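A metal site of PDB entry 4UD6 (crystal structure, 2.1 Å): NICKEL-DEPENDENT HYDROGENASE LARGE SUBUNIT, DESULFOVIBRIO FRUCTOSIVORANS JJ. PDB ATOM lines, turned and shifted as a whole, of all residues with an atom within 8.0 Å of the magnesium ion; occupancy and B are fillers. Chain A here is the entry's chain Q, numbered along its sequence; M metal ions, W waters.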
ATOM      1  N   PHE A  49      22.529  10.101 -20.610  1.00  0.00           N
ATOM      2  CA  PHE A  49      21.855   9.210 -19.662  1.00  0.00           C
ATOM      3  C   PHE A  49      22.344   9.497 -18.259  1.00  0.00           C
ATOM      4  O   PHE A  49      23.545   9.633 -18.046  1.00  0.00           O
ATOM      5  CB  PHE A  49      22.121   7.745 -20.010  1.00  0.00           C
ATOM      6  CG  PHE A  49      21.495   6.742 -19.065  1.00  0.00           C
ATOM      7  CD1 PHE A  49      20.190   6.318 -19.251  1.00  0.00           C
ATOM      8  CD2 PHE A  49      22.208   6.215 -18.009  1.00  0.00           C
ATOM      9  CE1 PHE A  49      19.614   5.362 -18.399  1.00  0.00           C
ATOM     10  CE2 PHE A  49      21.642   5.261 -17.154  1.00  0.00           C
ATOM     11  CZ  PHE A  49      20.328   4.864 -17.344  1.00  0.00           C
ATOM     12  N   GLU A  53      16.167   5.840 -12.329  1.00  0.00           N
ATOM     13  CA  GLU A  53      15.412   4.642 -11.976  1.00  0.00           C
ATOM     14  C   GLU A  53      16.356   3.596 -11.349  1.00  0.00           C
ATOM     15  O   GLU A  53      15.963   2.919 -10.429  1.00  0.00           O
ATOM     16  CB  GLU A  53      14.697   4.059 -13.200  1.00  0.00           C
ATOM     17  CG  GLU A  53      13.683   5.018 -13.819  1.00  0.00           C
ATOM     18  CD  GLU A  53      13.393   4.759 -15.282  1.00  0.00           C
ATOM     19  OE1 GLU A  53      14.272   4.217 -15.996  1.00  0.00           O
ATOM     20  OE2 GLU A  53      12.282   5.157 -15.709  1.00  0.00           O
ATOM     21  N   GLU A 334       6.732   0.485 -22.832  1.00  0.00           N
ATOM     22  CA  GLU A 334       7.896   1.111 -23.470  1.00  0.00           C
ATOM     23  C   GLU A 334       8.758   0.121 -24.212  1.00  0.00           C
ATOM     24  O   GLU A 334       9.045  -0.981 -23.699  1.00  0.00           O
ATOM     25  CB  GLU A 334       8.740   1.863 -22.435  1.00  0.00           C
ATOM     26  CG  GLU A 334       7.980   2.961 -21.724  1.00  0.00           C
ATOM     27  CD  GLU A 334       8.835   3.618 -20.651  1.00  0.00           C
ATOM     28  OE1 GLU A 334       9.101   2.960 -19.621  1.00  0.00           O
ATOM     29  OE2 GLU A 334       9.250   4.781 -20.840  1.00  0.00           O
ATOM     30  N   TYR A 341      19.625   0.394 -24.782  1.00  0.00           N
ATOM     31  CA  TYR A 341      19.331  -0.500 -23.656  1.00  0.00           C
ATOM     32  C   TYR A 341      19.535  -1.929 -24.154  1.00  0.00           C
ATOM     33  O   TYR A 341      19.538  -2.165 -25.338  1.00  0.00           O
ATOM     34  CB  TYR A 341      17.913  -0.286 -23.126  1.00  0.00           C
ATOM     35  CG  TYR A 341      17.750   1.135 -22.559  1.00  0.00           C
ATOM     36  CD1 TYR A 341      18.245   1.466 -21.288  1.00  0.00           C
ATOM     37  CD2 TYR A 341      17.141   2.138 -23.310  1.00  0.00           C
ATOM     38  CE1 TYR A 341      18.165   2.765 -20.810  1.00  0.00           C
ATOM     39  CE2 TYR A 341      17.064   3.424 -22.829  1.00  0.00           C
ATOM     40  CZ  TYR A 341      17.558   3.737 -21.573  1.00  0.00           C
ATOM     41  OH  TYR A 341      17.448   5.004 -21.107  1.00  0.00           O
ATOM     42  N   PRO A 350       5.166  -0.080 -17.401  1.00  0.00           N
ATOM     43  CA  PRO A 350       6.081   0.536 -16.428  1.00  0.00           C
ATOM     44  C   PRO A 350       6.186  -0.187 -15.085  1.00  0.00           C
ATOM     45  O   PRO A 350       7.220  -0.152 -14.484  1.00  0.00           O
ATOM     46  CB  PRO A 350       5.523   1.957 -16.247  1.00  0.00           C
ATOM     47  CG  PRO A 350       4.716   2.227 -17.458  1.00  0.00           C
ATOM     48  CD  PRO A 350       4.278   0.906 -18.040  1.00  0.00           C
ATOM     49  N   GLY A 353       8.933  -2.250 -15.716  1.00  0.00           N
ATOM     50  CA  GLY A 353       9.948  -1.573 -16.527  1.00  0.00           C
ATOM     51  C   GLY A 353      11.345  -2.118 -16.281  1.00  0.00           C
ATOM     52  O   GLY A 353      11.627  -2.606 -15.192  1.00  0.00           O
ATOM     53  N   VAL A 354      12.201  -2.077 -17.306  1.00  0.00           N
ATOM     54  CA  VAL A 354      13.599  -2.492 -17.200  1.00  0.00           C
ATOM     55  C   VAL A 354      14.434  -1.327 -17.750  1.00  0.00           C
ATOM     56  O   VAL A 354      14.094  -0.779 -18.814  1.00  0.00           O
ATOM     57  CB  VAL A 354      13.891  -3.816 -17.988  1.00  0.00           C
ATOM     58  CG1 VAL A 354      15.379  -4.154 -18.002  1.00  0.00           C
ATOM     59  CG2 VAL A 354      13.100  -4.971 -17.406  1.00  0.00           C
ATOM     60  N   THR A 355      15.500  -0.948 -17.037  1.00  0.00           N
ATOM     61  CA  THR A 355      16.437   0.097 -17.444  1.00  0.00           C
ATOM     62  C   THR A 355      17.863  -0.429 -17.389  1.00  0.00           C
ATOM     63  O   THR A 355      18.571  -0.294 -16.374  1.00  0.00           O
ATOM     64  CB  THR A 355      16.266   1.337 -16.546  1.00  0.00           C
ATOM     65  OG1 THR A 355      14.890   1.738 -16.588  1.00  0.00           O
ATOM     66  CG2 THR A 355      17.206   2.503 -16.996  1.00  0.00           C
ATOM     67  N   TRP A 370      19.005   7.529 -25.963  1.00  0.00           N
ATOM     68  CA  TRP A 370      18.939   7.156 -24.575  1.00  0.00           C
ATOM     69  C   TRP A 370      17.493   7.137 -24.054  1.00  0.00           C
ATOM     70  O   TRP A 370      17.232   6.615 -22.949  1.00  0.00           O
ATOM     71  CB  TRP A 370      19.827   8.081 -23.737  1.00  0.00           C
ATOM     72  CG  TRP A 370      21.276   7.700 -23.758  1.00  0.00           C
ATOM     73  CD1 TRP A 370      22.302   8.410 -24.297  1.00  0.00           C
ATOM     74  CD2 TRP A 370      21.848   6.502 -23.217  1.00  0.00           C
ATOM     75  NE1 TRP A 370      23.487   7.740 -24.120  1.00  0.00           N
ATOM     76  CE2 TRP A 370      23.238   6.557 -23.462  1.00  0.00           C
ATOM     77  CE3 TRP A 370      21.324   5.387 -22.546  1.00  0.00           C
ATOM     78  CZ2 TRP A 370      24.123   5.552 -23.057  1.00  0.00           C
ATOM     79  CZ3 TRP A 370      22.195   4.369 -22.151  1.00  0.00           C
ATOM     80  CH2 TRP A 370      23.573   4.465 -22.402  1.00  0.00           C
ATOM     81  N   MET A 371      16.552   7.719 -24.814  1.00  0.00           N
ATOM     82  CA  MET A 371      15.124   7.553 -24.528  1.00  0.00           C
ATOM     83  C   MET A 371      14.603   6.177 -24.959  1.00  0.00           C
ATOM     84  O   MET A 371      14.999   5.668 -26.004  1.00  0.00           O
ATOM     85  CB  MET A 371      14.279   8.654 -25.191  1.00  0.00           C
ATOM     86  CG  MET A 371      14.534  10.069 -24.655  1.00  0.00           C
ATOM     87  SD  MET A 371      13.191  11.172 -25.133  1.00  0.00           S
ATOM     88  CE  MET A 371      13.919  12.781 -24.764  1.00  0.00           C
ATOM     89  N   LYS A 372      13.729   5.619 -24.134  1.00  0.00           N
ATOM     90  CA  LYS A 372      12.866   4.513 -24.502  1.00  0.00           C
ATOM     91  C   LYS A 372      11.785   5.051 -25.434  1.00  0.00           C
ATOM     92  O   LYS A 372      11.651   6.254 -25.599  1.00  0.00           O
ATOM     93  CB  LYS A 372      12.239   3.861 -23.271  1.00  0.00           C
ATOM     94  CG  LYS A 372      13.237   3.467 -22.193  1.00  0.00           C
ATOM     95  CD  LYS A 372      12.573   2.667 -21.094  1.00  0.00           C
ATOM     96  CE  LYS A 372      13.595   2.127 -20.097  1.00  0.00           C
ATOM     97  NZ  LYS A 372      12.889   1.748 -18.822  1.00  0.00           N
ATOM     98  N   PRO A 374       7.931   5.006 -25.655  1.00  0.00           N
ATOM     99  CA  PRO A 374       6.613   4.685 -25.112  1.00  0.00           C
ATOM    100  C   PRO A 374       5.578   4.589 -26.213  1.00  0.00           C
ATOM    101  O   PRO A 374       5.555   5.416 -27.139  1.00  0.00           O
ATOM    102  CB  PRO A 374       6.261   5.917 -24.216  1.00  0.00           C
ATOM    103  CG  PRO A 374       7.566   6.644 -24.041  1.00  0.00           C
ATOM    104  CD  PRO A 374       8.297   6.403 -25.330  1.00  0.00           C
ATOM    105  N   SER A 480       3.865  10.042 -15.887  1.00  0.00           N
ATOM    106  CA  SER A 480       3.494   9.005 -14.925  1.00  0.00           C
ATOM    107  C   SER A 480       4.717   8.415 -14.246  1.00  0.00           C
ATOM    108  O   SER A 480       5.759   8.208 -14.887  1.00  0.00           O
ATOM    109  CB  SER A 480       2.608   7.907 -15.570  1.00  0.00           C
ATOM    110  OG  SER A 480       3.222   7.337 -16.724  1.00  0.00           O
ATOM    111  N   TRP A 482       5.755   5.206 -11.577  1.00  0.00           N
ATOM    112  CA  TRP A 482       5.242   3.896 -11.272  1.00  0.00           C
ATOM    113  C   TRP A 482       6.168   3.187 -10.267  1.00  0.00           C
ATOM    114  O   TRP A 482       7.362   3.002 -10.534  1.00  0.00           O
ATOM    115  CB  TRP A 482       5.172   3.079 -12.565  1.00  0.00           C
ATOM    116  CG  TRP A 482       4.466   3.747 -13.752  1.00  0.00           C
ATOM    117  CD1 TRP A 482       4.971   4.707 -14.587  1.00  0.00           C
ATOM    118  CD2 TRP A 482       3.157   3.428 -14.253  1.00  0.00           C
ATOM    119  NE1 TRP A 482       4.047   5.009 -15.574  1.00  0.00           N
ATOM    120  CE2 TRP A 482       2.923   4.253 -15.379  1.00  0.00           C
ATOM    121  CE3 TRP A 482       2.130   2.569 -13.822  1.00  0.00           C
ATOM    122  CZ2 TRP A 482       1.711   4.216 -16.091  1.00  0.00           C
ATOM    123  CZ3 TRP A 482       0.949   2.534 -14.533  1.00  0.00           C
ATOM    124  CH2 TRP A 482       0.748   3.349 -15.643  1.00  0.00           C
ATOM    125  N   PHE A 493      11.060   1.479  -9.739  1.00  0.00           N
ATOM    126  CA  PHE A 493      10.527   2.820  -9.869  1.00  0.00           C
ATOM    127  C   PHE A 493      10.797   3.273 -11.275  1.00  0.00           C
ATOM    128  O   PHE A 493      11.951   3.353 -11.700  1.00  0.00           O
ATOM    129  CB  PHE A 493      11.167   3.789  -8.871  1.00  0.00           C
ATOM    130  CG  PHE A 493      10.327   4.995  -8.611  1.00  0.00           C
ATOM    131  CD1 PHE A 493      10.208   5.998  -9.558  1.00  0.00           C
ATOM    132  CD2 PHE A 493       9.581   5.097  -7.434  1.00  0.00           C
ATOM    133  CE1 PHE A 493       9.393   7.105  -9.314  1.00  0.00           C
ATOM    134  CE2 PHE A 493       8.762   6.187  -7.191  1.00  0.00           C
ATOM    135  CZ  PHE A 493       8.665   7.190  -8.139  1.00  0.00           C
ATOM    136  N   GLN A 494       9.750   3.566 -12.009  1.00  0.00           N
ATOM    137  CA  GLN A 494       9.860   3.889 -13.426  1.00  0.00           C
ATOM    138  C   GLN A 494       9.140   5.190 -13.711  1.00  0.00           C
ATOM    139  O   GLN A 494       8.017   5.385 -13.259  1.00  0.00           O
ATOM    140  CB  GLN A 494       9.242   2.776 -14.271  1.00  0.00           C
ATOM    141  CG  GLN A 494       9.996   1.456 -14.144  1.00  0.00           C
ATOM    142  CD  GLN A 494      11.298   1.448 -14.928  1.00  0.00           C
ATOM    143  OE1 GLN A 494      11.386   2.043 -15.994  1.00  0.00           O
ATOM    144  NE2 GLN A 494      12.305   0.766 -14.394  1.00  0.00           N
ATOM    145  N   LEU A 495       9.823   6.061 -14.443  1.00  0.00           N
ATOM    146  CA  LEU A 495       9.300   7.323 -14.961  1.00  0.00           C
ATOM    147  C   LEU A 495       9.015   7.136 -16.457  1.00  0.00           C
ATOM    148  O   LEU A 495       9.881   6.604 -17.175  1.00  0.00           O
ATOM    149  CB  LEU A 495      10.339   8.438 -14.798  1.00  0.00           C
ATOM    150  CG  LEU A 495      10.708   8.914 -13.378  1.00  0.00           C
ATOM    151  CD1 LEU A 495      11.565   7.923 -12.601  1.00  0.00           C
ATOM    152  CD2 LEU A 495      11.409  10.250 -13.424  1.00  0.00           C
ATOM    153  N   VAL A 496       7.814   7.521 -16.892  1.00  0.00           N
ATOM    154  CA  VAL A 496       7.463   7.668 -18.307  1.00  0.00           C
ATOM    155  C   VAL A 496       7.024   9.119 -18.441  1.00  0.00           C
ATOM    156  O   VAL A 496       6.042   9.526 -17.834  1.00  0.00           O
ATOM    157  CB  VAL A 496       6.326   6.718 -18.784  1.00  0.00           C
ATOM    158  CG1 VAL A 496       6.222   6.724 -20.310  1.00  0.00           C
ATOM    159  CG2 VAL A 496       6.574   5.280 -18.363  1.00  0.00           C
ATOM    160  N   VAL A 497       7.772   9.898 -19.225  1.00  0.00           N
ATOM    161  CA  VAL A 497       7.772  11.337 -19.099  1.00  0.00           C
ATOM    162  C   VAL A 497       7.333  11.893 -20.438  1.00  0.00           C
ATOM    163  O   VAL A 497       7.549  11.252 -21.455  1.00  0.00           O
ATOM    164  CB  VAL A 497       9.156  11.828 -18.655  1.00  0.00           C
ATOM    165  CG1 VAL A 497       9.128  13.318 -18.255  1.00  0.00           C
ATOM    166  CG2 VAL A 497       9.597  11.001 -17.446  1.00  0.00           C
ATOM    167  N   THR A 500       9.576  11.727 -23.288  1.00  0.00           N
ATOM    168  CA  THR A 500       9.808  10.355 -23.753  1.00  0.00           C
ATOM    169  C   THR A 500       8.773   9.991 -24.802  1.00  0.00           C
ATOM    170  O   THR A 500       9.118   9.383 -25.810  1.00  0.00           O
ATOM    171  CB  THR A 500       9.727   9.296 -22.613  1.00  0.00           C
ATOM    172  OG1 THR A 500      10.281   9.822 -21.405  1.00  0.00           O
ATOM    173  CG2 THR A 500      10.493   8.056 -23.014  1.00  0.00           C
ATOM    174  N   CYS A 546      14.317  15.168 -18.815  1.00  0.00           N
ATOM    175  CA  CYS A 546      13.014  14.551 -18.514  1.00  0.00           C
ATOM    176  C   CYS A 546      12.849  13.233 -19.296  1.00  0.00           C
ATOM    177  O   CYS A 546      12.501  12.186 -18.730  1.00  0.00           O
ATOM    178  CB  CYS A 546      11.869  15.492 -18.872  1.00  0.00           C
ATOM    179  SG  CYS A 546      11.264  16.459 -17.499  1.00  0.00           S
ATOM    180  N   GLY A 547      13.095  13.292 -20.597  1.00  0.00           N
ATOM    181  CA  GLY A 547      12.815  12.164 -21.479  1.00  0.00           C
ATOM    182  C   GLY A 547      13.593  10.922 -21.109  1.00  0.00           C
ATOM    183  O   GLY A 547      13.031   9.833 -21.085  1.00  0.00           O
ATOM    184  N   VAL A 548      14.887  11.105 -20.809  1.00  0.00           N
ATOM    185  CA  VAL A 548      15.796  10.010 -20.465  1.00  0.00           C
ATOM    186  C   VAL A 548      15.808   9.676 -18.957  1.00  0.00           C
ATOM    187  O   VAL A 548      15.736   8.498 -18.598  1.00  0.00           O
ATOM    188  CB  VAL A 548      17.238  10.349 -20.919  1.00  0.00           C
ATOM    189  CG1 VAL A 548      18.175   9.222 -20.603  1.00  0.00           C
ATOM    190  CG2 VAL A 548      17.300  10.695 -22.394  1.00  0.00           C
ATOM    191  N   HIS A 549      15.902  10.701 -18.102  1.00  0.00           N
ATOM    192  CA  HIS A 549      16.097  10.535 -16.645  1.00  0.00           C
ATOM    193  C   HIS A 549      17.232   9.526 -16.329  1.00  0.00           C
ATOM    194  O   HIS A 549      17.169   8.619 -15.479  1.00  0.00           O
ATOM    195  CB  HIS A 549      14.778  10.246 -15.870  1.00  0.00           C
ATOM    196  CG  HIS A 549      13.844   9.303 -16.580  1.00  0.00           C
ATOM    197  ND1 HIS A 549      13.037   9.714 -17.625  1.00  0.00           N
ATOM    198  CD2 HIS A 549      13.651   7.968 -16.447  1.00  0.00           C
ATOM    199  CE1 HIS A 549      12.368   8.676 -18.085  1.00  0.00           C
ATOM    200  NE2 HIS A 549      12.723   7.598 -17.388  1.00  0.00           N
ATOM    201  OXT HIS A 549      18.308   9.646 -16.937  1.00  0.00           O
HETATM  202 MG    MG M   1      11.754   5.647 -17.718  1.00  0.00          MG
HETATM  203  O   HOH W   1      11.270   6.102 -19.639  1.00  0.00           O
HETATM  204  O   HOH W   2      10.835   3.882 -17.885  1.00  0.00           O
HETATM  205  O   HOH W   3      13.480   4.812 -18.452  1.00  0.00           O
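The magnesium ion is bound by water W2 (2.0 Å). Water W1 is bound to the magnesium ion (2.0 Å). Water W3 is bound to the magnesium ion (2.1 Å). OE2 of Glu 53 is bound to the magnesium ion, 2.1 Å away. O of Leu 495 is bound to the magnesium ion (2.2 Å). NE2 of His 549 is bound to the magnesium ion (2.2 Å). The magnesium ion has six donor atoms within binding distance.
Water W2 lies within hydrogen-bond range of OE1 of Glu 334 (2.6 Å), OE1 of Gln 494 (2.7 Å) and NZ of Lys 372 (3.1 Å). Water W3 bridges OE1 of Glu 53 and NZ of Lys 372.
Within 4 Å of the magnesium ion: Glu 53, Leu 495 and His 549. Along chain A the residues within 4 Å of the magnesium ion span positions 53 to 549. The nearest printed residue that does not touch the magnesium ion is Gln 494 (4.01 Å).
The side-chain carboxylate (OE2) of Glu 53 lies close to the side-chain amide oxygen (OE1) of Gln 494 (3.3 Å). OE1 of Glu 53 lies within salt-bridge range of NZ of Lys 372 (3.999 Å). The side-chain carboxylate of Glu 53 is in hydrogen-bond range of the side-chain hydroxyl of Thr 355, 2.6 Å away. ND1 of His 549 lies close to O of Gly 547, 3.5 Å away. A ring nitrogen (ND1) of His 549 lies within hydrogen-bond range of the backbone carbonyl oxygen (O) of Cys 546 (2.8 Å).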
